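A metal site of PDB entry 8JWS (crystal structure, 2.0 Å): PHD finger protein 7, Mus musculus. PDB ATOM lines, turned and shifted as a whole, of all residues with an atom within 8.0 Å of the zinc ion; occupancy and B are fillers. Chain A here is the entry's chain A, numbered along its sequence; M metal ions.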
ATOM      1  N   VAL A  10       0.035 -32.220  19.750  1.00  0.00           N
ATOM      2  CA  VAL A  10      -0.477 -31.691  21.019  1.00  0.00           C
ATOM      3  C   VAL A  10      -0.463 -30.148  21.129  1.00  0.00           C
ATOM      4  O   VAL A  10       0.318 -29.481  20.478  1.00  0.00           O
ATOM      5  CB  VAL A  10       0.274 -32.281  22.250  1.00  0.00           C
ATOM      6  CG1 VAL A  10       0.232 -33.800  22.238  1.00  0.00           C
ATOM      7  CG2 VAL A  10       1.689 -31.765  22.329  1.00  0.00           C
ATOM      8  N   CYS A  11      -1.346 -29.612  21.942  1.00  0.00           N
ATOM      9  CA  CYS A  11      -1.392 -28.180  22.182  1.00  0.00           C
ATOM     10  C   CYS A  11      -0.156 -27.756  22.974  1.00  0.00           C
ATOM     11  O   CYS A  11       0.166 -28.349  23.999  1.00  0.00           O
ATOM     12  CB  CYS A  11      -2.691 -27.858  22.904  1.00  0.00           C
ATOM     13  SG  CYS A  11      -2.812 -26.191  23.580  1.00  0.00           S
ATOM     14  N   LEU A  12       0.493 -26.691  22.503  1.00  0.00           N
ATOM     15  CA  LEU A  12       1.686 -26.129  23.116  1.00  0.00           C
ATOM     16  C   LEU A  12       1.441 -25.598  24.539  1.00  0.00           C
ATOM     17  O   LEU A  12       2.362 -25.588  25.362  1.00  0.00           O
ATOM     18  CB  LEU A  12       2.156 -24.995  22.194  1.00  0.00           C
ATOM     19  CG  LEU A  12       3.495 -24.342  22.548  1.00  0.00           C
ATOM     20  CD1 LEU A  12       4.632 -25.248  22.209  1.00  0.00           C
ATOM     21  CD2 LEU A  12       3.636 -23.040  21.821  1.00  0.00           C
ATOM     22  N   LEU A  13       0.206 -25.185  24.816  1.00  0.00           N
ATOM     23  CA  LEU A  13      -0.147 -24.543  26.088  1.00  0.00           C
ATOM     24  C   LEU A  13      -0.622 -25.530  27.159  1.00  0.00           C
ATOM     25  O   LEU A  13      -0.253 -25.390  28.320  1.00  0.00           O
ATOM     26  CB  LEU A  13      -1.212 -23.475  25.831  1.00  0.00           C
ATOM     27  CG  LEU A  13      -0.725 -22.258  25.012  1.00  0.00           C
ATOM     28  CD1 LEU A  13      -1.827 -21.254  24.811  1.00  0.00           C
ATOM     29  CD2 LEU A  13       0.456 -21.577  25.688  1.00  0.00           C
ATOM     30  N   CYS A  14      -1.454 -26.517  26.786  1.00  0.00           N
ATOM     31  CA  CYS A  14      -1.920 -27.494  27.751  1.00  0.00           C
ATOM     32  C   CYS A  14      -1.236 -28.858  27.629  1.00  0.00           C
ATOM     33  O   CYS A  14      -1.387 -29.691  28.507  1.00  0.00           O
ATOM     34  CB  CYS A  14      -3.445 -27.645  27.695  1.00  0.00           C
ATOM     35  SG  CYS A  14      -4.053 -28.539  26.258  1.00  0.00           S
ATOM     36  N   LEU A  15      -0.519 -29.074  26.529  1.00  0.00           N
ATOM     37  CA  LEU A  15       0.241 -30.290  26.246  1.00  0.00           C
ATOM     38  C   LEU A  15      -0.633 -31.518  25.985  1.00  0.00           C
ATOM     39  O   LEU A  15      -0.127 -32.636  26.007  1.00  0.00           O
ATOM     40  CB  LEU A  15       1.236 -30.551  27.395  1.00  0.00           C
ATOM     41  CG  LEU A  15       2.130 -29.378  27.762  1.00  0.00           C
ATOM     42  CD1 LEU A  15       2.987 -29.723  28.994  1.00  0.00           C
ATOM     43  CD2 LEU A  15       3.020 -29.001  26.608  1.00  0.00           C
ATOM     44  N   GLN A  16      -1.933 -31.301  25.734  1.00  0.00           N
ATOM     45  CA  GLN A  16      -2.853 -32.392  25.459  1.00  0.00           C
ATOM     46  C   GLN A  16      -3.289 -32.461  23.992  1.00  0.00           C
ATOM     47  O   GLN A  16      -3.115 -31.519  23.231  1.00  0.00           O
ATOM     48  CB  GLN A  16      -4.109 -32.276  26.326  1.00  0.00           C
ATOM     49  CG  GLN A  16      -3.781 -32.502  27.825  1.00  0.00           C
ATOM     50  CD  GLN A  16      -5.011 -32.754  28.650  1.00  0.00           C
ATOM     51  OE1 GLN A  16      -6.059 -33.173  28.104  1.00  0.00           O
ATOM     52  NE2 GLN A  16      -4.888 -32.537  29.946  1.00  0.00           N
ATOM     53  N   GLU A  17      -3.884 -33.596  23.636  1.00  0.00           N
ATOM     54  CA  GLU A  17      -4.347 -33.847  22.286  1.00  0.00           C
ATOM     55  C   GLU A  17      -5.616 -33.039  22.010  1.00  0.00           C
ATOM     56  O   GLU A  17      -6.173 -32.441  22.932  1.00  0.00           O
ATOM     57  CB  GLU A  17      -4.558 -35.356  22.116  1.00  0.00           C
ATOM     58  CG  GLU A  17      -3.227 -36.103  22.057  1.00  0.00           C
ATOM     59  CD  GLU A  17      -3.319 -37.613  22.042  1.00  0.00           C
ATOM     60  OE1 GLU A  17      -4.042 -38.155  22.909  1.00  0.00           O
ATOM     61  OE2 GLU A  17      -2.672 -38.263  21.185  1.00  0.00           O
ATOM     62  N   PRO A  18      -6.071 -32.962  20.743  1.00  0.00           N
ATOM     63  CA  PRO A  18      -7.204 -32.086  20.379  1.00  0.00           C
ATOM     64  C   PRO A  18      -8.403 -32.198  21.303  1.00  0.00           C
ATOM     65  O   PRO A  18      -8.915 -31.179  21.759  1.00  0.00           O
ATOM     66  CB  PRO A  18      -7.509 -32.530  18.944  1.00  0.00           C
ATOM     67  CG  PRO A  18      -6.129 -32.925  18.405  1.00  0.00           C
ATOM     68  CD  PRO A  18      -5.501 -33.653  19.566  1.00  0.00           C
ATOM     69  N   LEU A  24     -12.509 -27.290  24.751  1.00  0.00           N
ATOM     70  CA  LEU A  24     -11.196 -26.698  24.564  1.00  0.00           C
ATOM     71  C   LEU A  24     -11.091 -25.837  23.297  1.00  0.00           C
ATOM     72  O   LEU A  24     -10.080 -25.177  23.082  1.00  0.00           O
ATOM     73  CB  LEU A  24     -10.159 -27.821  24.485  1.00  0.00           C
ATOM     74  CG  LEU A  24     -10.074 -28.735  25.713  1.00  0.00           C
ATOM     75  CD1 LEU A  24      -9.042 -29.838  25.505  1.00  0.00           C
ATOM     76  CD2 LEU A  24      -9.688 -27.996  26.879  1.00  0.00           C
ATOM     77  N   GLY A  25     -12.139 -25.873  22.470  1.00  0.00           N
ATOM     78  CA  GLY A  25     -12.144 -25.144  21.216  1.00  0.00           C
ATOM     79  C   GLY A  25     -11.422 -25.947  20.129  1.00  0.00           C
ATOM     80  O   GLY A  25     -10.795 -26.964  20.425  1.00  0.00           O
ATOM     81  N   GLU A  26     -11.540 -25.464  18.895  1.00  0.00           N
ATOM     82  CA  GLU A  26     -10.862 -26.095  17.765  1.00  0.00           C
ATOM     83  C   GLU A  26      -9.359 -26.148  17.997  1.00  0.00           C
ATOM     84  O   GLU A  26      -8.772 -25.244  18.596  1.00  0.00           O
ATOM     85  CB  GLU A  26     -11.134 -25.324  16.469  1.00  0.00           C
ATOM     86  CG  GLU A  26     -12.562 -25.438  15.960  1.00  0.00           C
ATOM     87  CD  GLU A  26     -12.943 -26.804  15.435  1.00  0.00           C
ATOM     88  OE1 GLU A  26     -12.353 -27.252  14.414  1.00  0.00           O
ATOM     89  OE2 GLU A  26     -13.843 -27.425  16.053  1.00  0.00           O
ATOM     90  N   PHE A  27      -8.741 -27.219  17.492  1.00  0.00           N
ATOM     91  CA  PHE A  27      -7.310 -27.386  17.494  1.00  0.00           C
ATOM     92  C   PHE A  27      -6.742 -26.674  16.265  1.00  0.00           C
ATOM     93  O   PHE A  27      -7.040 -27.023  15.125  1.00  0.00           O
ATOM     94  CB  PHE A  27      -7.033 -28.881  17.466  1.00  0.00           C
ATOM     95  CG  PHE A  27      -5.624 -29.264  17.769  1.00  0.00           C
ATOM     96  CD1 PHE A  27      -5.123 -29.162  19.053  1.00  0.00           C
ATOM     97  CD2 PHE A  27      -4.780 -29.716  16.759  1.00  0.00           C
ATOM     98  CE1 PHE A  27      -3.804 -29.496  19.334  1.00  0.00           C
ATOM     99  CE2 PHE A  27      -3.470 -30.071  17.045  1.00  0.00           C
ATOM    100  CZ  PHE A  27      -2.996 -29.957  18.316  1.00  0.00           C
ATOM    101  N   CYS A  34       0.896 -25.713  17.270  1.00  0.00           N
ATOM    102  CA  CYS A  34      -0.411 -26.330  17.505  1.00  0.00           C
ATOM    103  C   CYS A  34      -0.952 -25.826  18.842  1.00  0.00           C
ATOM    104  O   CYS A  34      -0.240 -25.847  19.838  1.00  0.00           O
ATOM    105  CB  CYS A  34      -0.312 -27.850  17.504  1.00  0.00           C
ATOM    106  SG  CYS A  34       0.578 -28.554  16.104  1.00  0.00           S
ATOM    107  N   VAL A  35      -2.236 -25.425  18.864  1.00  0.00           N
ATOM    108  CA  VAL A  35      -2.838 -24.859  20.062  1.00  0.00           C
ATOM    109  C   VAL A  35      -4.354 -24.967  19.974  1.00  0.00           C
ATOM    110  O   VAL A  35      -4.928 -24.802  18.902  1.00  0.00           O
ATOM    111  CB  VAL A  35      -2.381 -23.375  20.311  1.00  0.00           C
ATOM    112  CG1 VAL A  35      -2.834 -22.452  19.193  1.00  0.00           C
ATOM    113  CG2 VAL A  35      -2.844 -22.864  21.656  1.00  0.00           C
ATOM    114  N   HIS A  36      -4.972 -25.237  21.123  1.00  0.00           N
ATOM    115  CA  HIS A  36      -6.421 -25.158  21.236  1.00  0.00           C
ATOM    116  C   HIS A  36      -6.840 -23.698  21.221  1.00  0.00           C
ATOM    117  O   HIS A  36      -6.170 -22.855  21.816  1.00  0.00           O
ATOM    118  CB  HIS A  36      -6.923 -25.755  22.550  1.00  0.00           C
ATOM    119  CG  HIS A  36      -6.746 -27.221  22.689  1.00  0.00           C
ATOM    120  ND1 HIS A  36      -5.920 -27.766  23.641  1.00  0.00           N
ATOM    121  CD2 HIS A  36      -7.363 -28.233  22.065  1.00  0.00           C
ATOM    122  CE1 HIS A  36      -5.999 -29.090  23.528  1.00  0.00           C
ATOM    123  NE2 HIS A  36      -6.876 -29.371  22.587  1.00  0.00           N
ATOM    124  N   TYR A  37      -7.972 -23.404  20.570  1.00  0.00           N
ATOM    125  CA  TYR A  37      -8.435 -22.023  20.523  1.00  0.00           C
ATOM    126  C   TYR A  37      -8.756 -21.463  21.908  1.00  0.00           C
ATOM    127  O   TYR A  37      -8.457 -20.291  22.203  1.00  0.00           O
ATOM    128  CB  TYR A  37      -9.656 -21.909  19.607  1.00  0.00           C
ATOM    129  CG  TYR A  37     -10.145 -20.488  19.488  1.00  0.00           C
ATOM    130  CD1 TYR A  37      -9.286 -19.468  19.090  1.00  0.00           C
ATOM    131  CD2 TYR A  37     -11.461 -20.157  19.806  1.00  0.00           C
ATOM    132  CE1 TYR A  37      -9.722 -18.160  18.990  1.00  0.00           C
ATOM    133  CE2 TYR A  37     -11.912 -18.849  19.706  1.00  0.00           C
ATOM    134  CZ  TYR A  37     -11.053 -17.867  19.276  1.00  0.00           C
ATOM    135  OH  TYR A  37     -11.504 -16.593  19.153  1.00  0.00           O
ATOM    136  N   PHE A  38      -9.359 -22.268  22.789  1.00  0.00           N
ATOM    137  CA  PHE A  38      -9.688 -21.773  24.118  1.00  0.00           C
ATOM    138  C   PHE A  38      -8.447 -21.638  24.983  1.00  0.00           C
ATOM    139  O   PHE A  38      -8.378 -20.736  25.829  1.00  0.00           O
ATOM    140  CB  PHE A  38     -10.743 -22.603  24.840  1.00  0.00           C
ATOM    141  CG  PHE A  38     -12.105 -22.651  24.222  1.00  0.00           C
ATOM    142  CD1 PHE A  38     -12.434 -21.837  23.152  1.00  0.00           C
ATOM    143  CD2 PHE A  38     -13.066 -23.487  24.729  1.00  0.00           C
ATOM    144  CE1 PHE A  38     -13.705 -21.916  22.563  1.00  0.00           C
ATOM    145  CE2 PHE A  38     -14.330 -23.553  24.166  1.00  0.00           C
ATOM    146  CZ  PHE A  38     -14.632 -22.774  23.075  1.00  0.00           C
ATOM    147  N   CYS A  39      -7.451 -22.507  24.778  1.00  0.00           N
ATOM    148  CA  CYS A  39      -6.192 -22.340  25.480  1.00  0.00           C
ATOM    149  C   CYS A  39      -5.565 -20.997  25.124  1.00  0.00           C
ATOM    150  O   CYS A  39      -5.015 -20.331  25.989  1.00  0.00           O
ATOM    151  CB  CYS A  39      -5.233 -23.507  25.247  1.00  0.00           C
ATOM    152  SG  CYS A  39      -5.736 -25.049  26.075  1.00  0.00           S
ATOM    153  N   LEU A  40      -5.684 -20.565  23.862  1.00  0.00           N
ATOM    154  CA  LEU A  40      -5.226 -19.264  23.434  1.00  0.00           C
ATOM    155  C   LEU A  40      -5.934 -18.083  24.107  1.00  0.00           C
ATOM    156  O   LEU A  40      -5.277 -17.196  24.701  1.00  0.00           O
ATOM    157  CB  LEU A  40      -5.422 -19.113  21.912  1.00  0.00           C
ATOM    158  CG  LEU A  40      -4.341 -19.423  20.950  1.00  0.00           C
ATOM    159  CD1 LEU A  40      -4.768 -18.934  19.528  1.00  0.00           C
ATOM    160  CD2 LEU A  40      -3.081 -18.797  21.331  1.00  0.00           C
ATOM    161  N   ILE A  86      -2.937 -21.176  32.810  1.00  0.00           N
ATOM    162  CA  ILE A  86      -4.059 -20.444  33.358  1.00  0.00           C
ATOM    163  C   ILE A  86      -3.954 -20.271  34.881  1.00  0.00           C
ATOM    164  O   ILE A  86      -3.682 -21.217  35.592  1.00  0.00           O
ATOM    165  CB  ILE A  86      -5.418 -21.053  32.972  1.00  0.00           C
ATOM    166  CG1 ILE A  86      -5.541 -21.116  31.452  1.00  0.00           C
ATOM    167  CG2 ILE A  86      -6.553 -20.247  33.584  1.00  0.00           C
ATOM    168  CD1 ILE A  86      -6.645 -22.025  30.977  1.00  0.00           C
ATOM    169  N   HIS A  98      -3.641 -26.341  33.708  1.00  0.00           N
ATOM    170  CA  HIS A  98      -3.926 -26.574  32.302  1.00  0.00           C
ATOM    171  C   HIS A  98      -5.444 -26.520  32.132  1.00  0.00           C
ATOM    172  O   HIS A  98      -6.174 -27.078  32.961  1.00  0.00           O
ATOM    173  CB  HIS A  98      -3.402 -27.935  31.849  1.00  0.00           C
ATOM    174  CG  HIS A  98      -1.948 -28.214  32.106  1.00  0.00           C
ATOM    175  ND1 HIS A  98      -1.530 -29.208  32.963  1.00  0.00           N
ATOM    176  CD2 HIS A  98      -0.832 -27.667  31.599  1.00  0.00           C
ATOM    177  CE1 HIS A  98      -0.186 -29.230  32.980  1.00  0.00           C
ATOM    178  NE2 HIS A  98       0.250 -28.303  32.161  1.00  0.00           N
ATOM    179  N   LEU A  99      -5.934 -25.891  31.057  1.00  0.00           N
ATOM    180  CA  LEU A  99      -7.380 -25.794  30.835  1.00  0.00           C
ATOM    181  C   LEU A  99      -8.133 -27.113  30.979  1.00  0.00           C
ATOM    182  O   LEU A  99      -9.082 -27.188  31.759  1.00  0.00           O
ATOM    183  CB  LEU A  99      -7.684 -25.174  29.454  1.00  0.00           C
ATOM    184  CG  LEU A  99      -9.140 -24.986  29.127  1.00  0.00           C
ATOM    185  CD1 LEU A  99      -9.797 -24.135  30.150  1.00  0.00           C
ATOM    186  CD2 LEU A  99      -9.324 -24.373  27.706  1.00  0.00           C
ATOM    187  N   PRO A 100      -7.747 -28.208  30.263  1.00  0.00           N
ATOM    188  CA  PRO A 100      -8.457 -29.490  30.387  1.00  0.00           C
ATOM    189  C   PRO A 100      -8.491 -30.044  31.814  1.00  0.00           C
ATOM    190  O   PRO A 100      -9.486 -30.607  32.242  1.00  0.00           O
ATOM    191  CB  PRO A 100      -7.704 -30.414  29.433  1.00  0.00           C
ATOM    192  CG  PRO A 100      -6.401 -29.707  29.124  1.00  0.00           C
ATOM    193  CD  PRO A 100      -6.617 -28.266  29.320  1.00  0.00           C
HETATM  194 ZN    ZN M   1      -4.678 -26.758  24.936  1.00  0.00          ZN
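The backbone carbonyl oxygen of Glu 17 lies within hydrogen-bond range of a ring nitrogen (NE2) of His 36 (3.2 Å).
O of Pro 18 lies within hydrogen-bond range of NE2 of His 36 (2.8 Å).
The backbone NH (N) of Gln 16 sits close to the side-chain sulfur (SG) of Cys 14, at 3.5 Å.
The backbone NH (N) of Leu 13 sits close to the side-chain sulfur (SG) of Cys 11 (3.4 Å).
The backbone NH of Cys 11 lies within hydrogen-bond range of the backbone carbonyl oxygen of Gln 16, at 2.9 Å.
ND1 of His 36 is bound to the zinc ion (2.1 Å).
The zinc ion is bound by SG of Cys 14 (2.3 Å).
SG of Cys 39 binds the zinc ion (2.3 Å).
The zinc ion is bound by the side-chain sulfur (SG) of Cys 11 (2.4 Å).
The nearest printed residue that does not touch the zinc ion is Leu 13 (4.8 Å).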
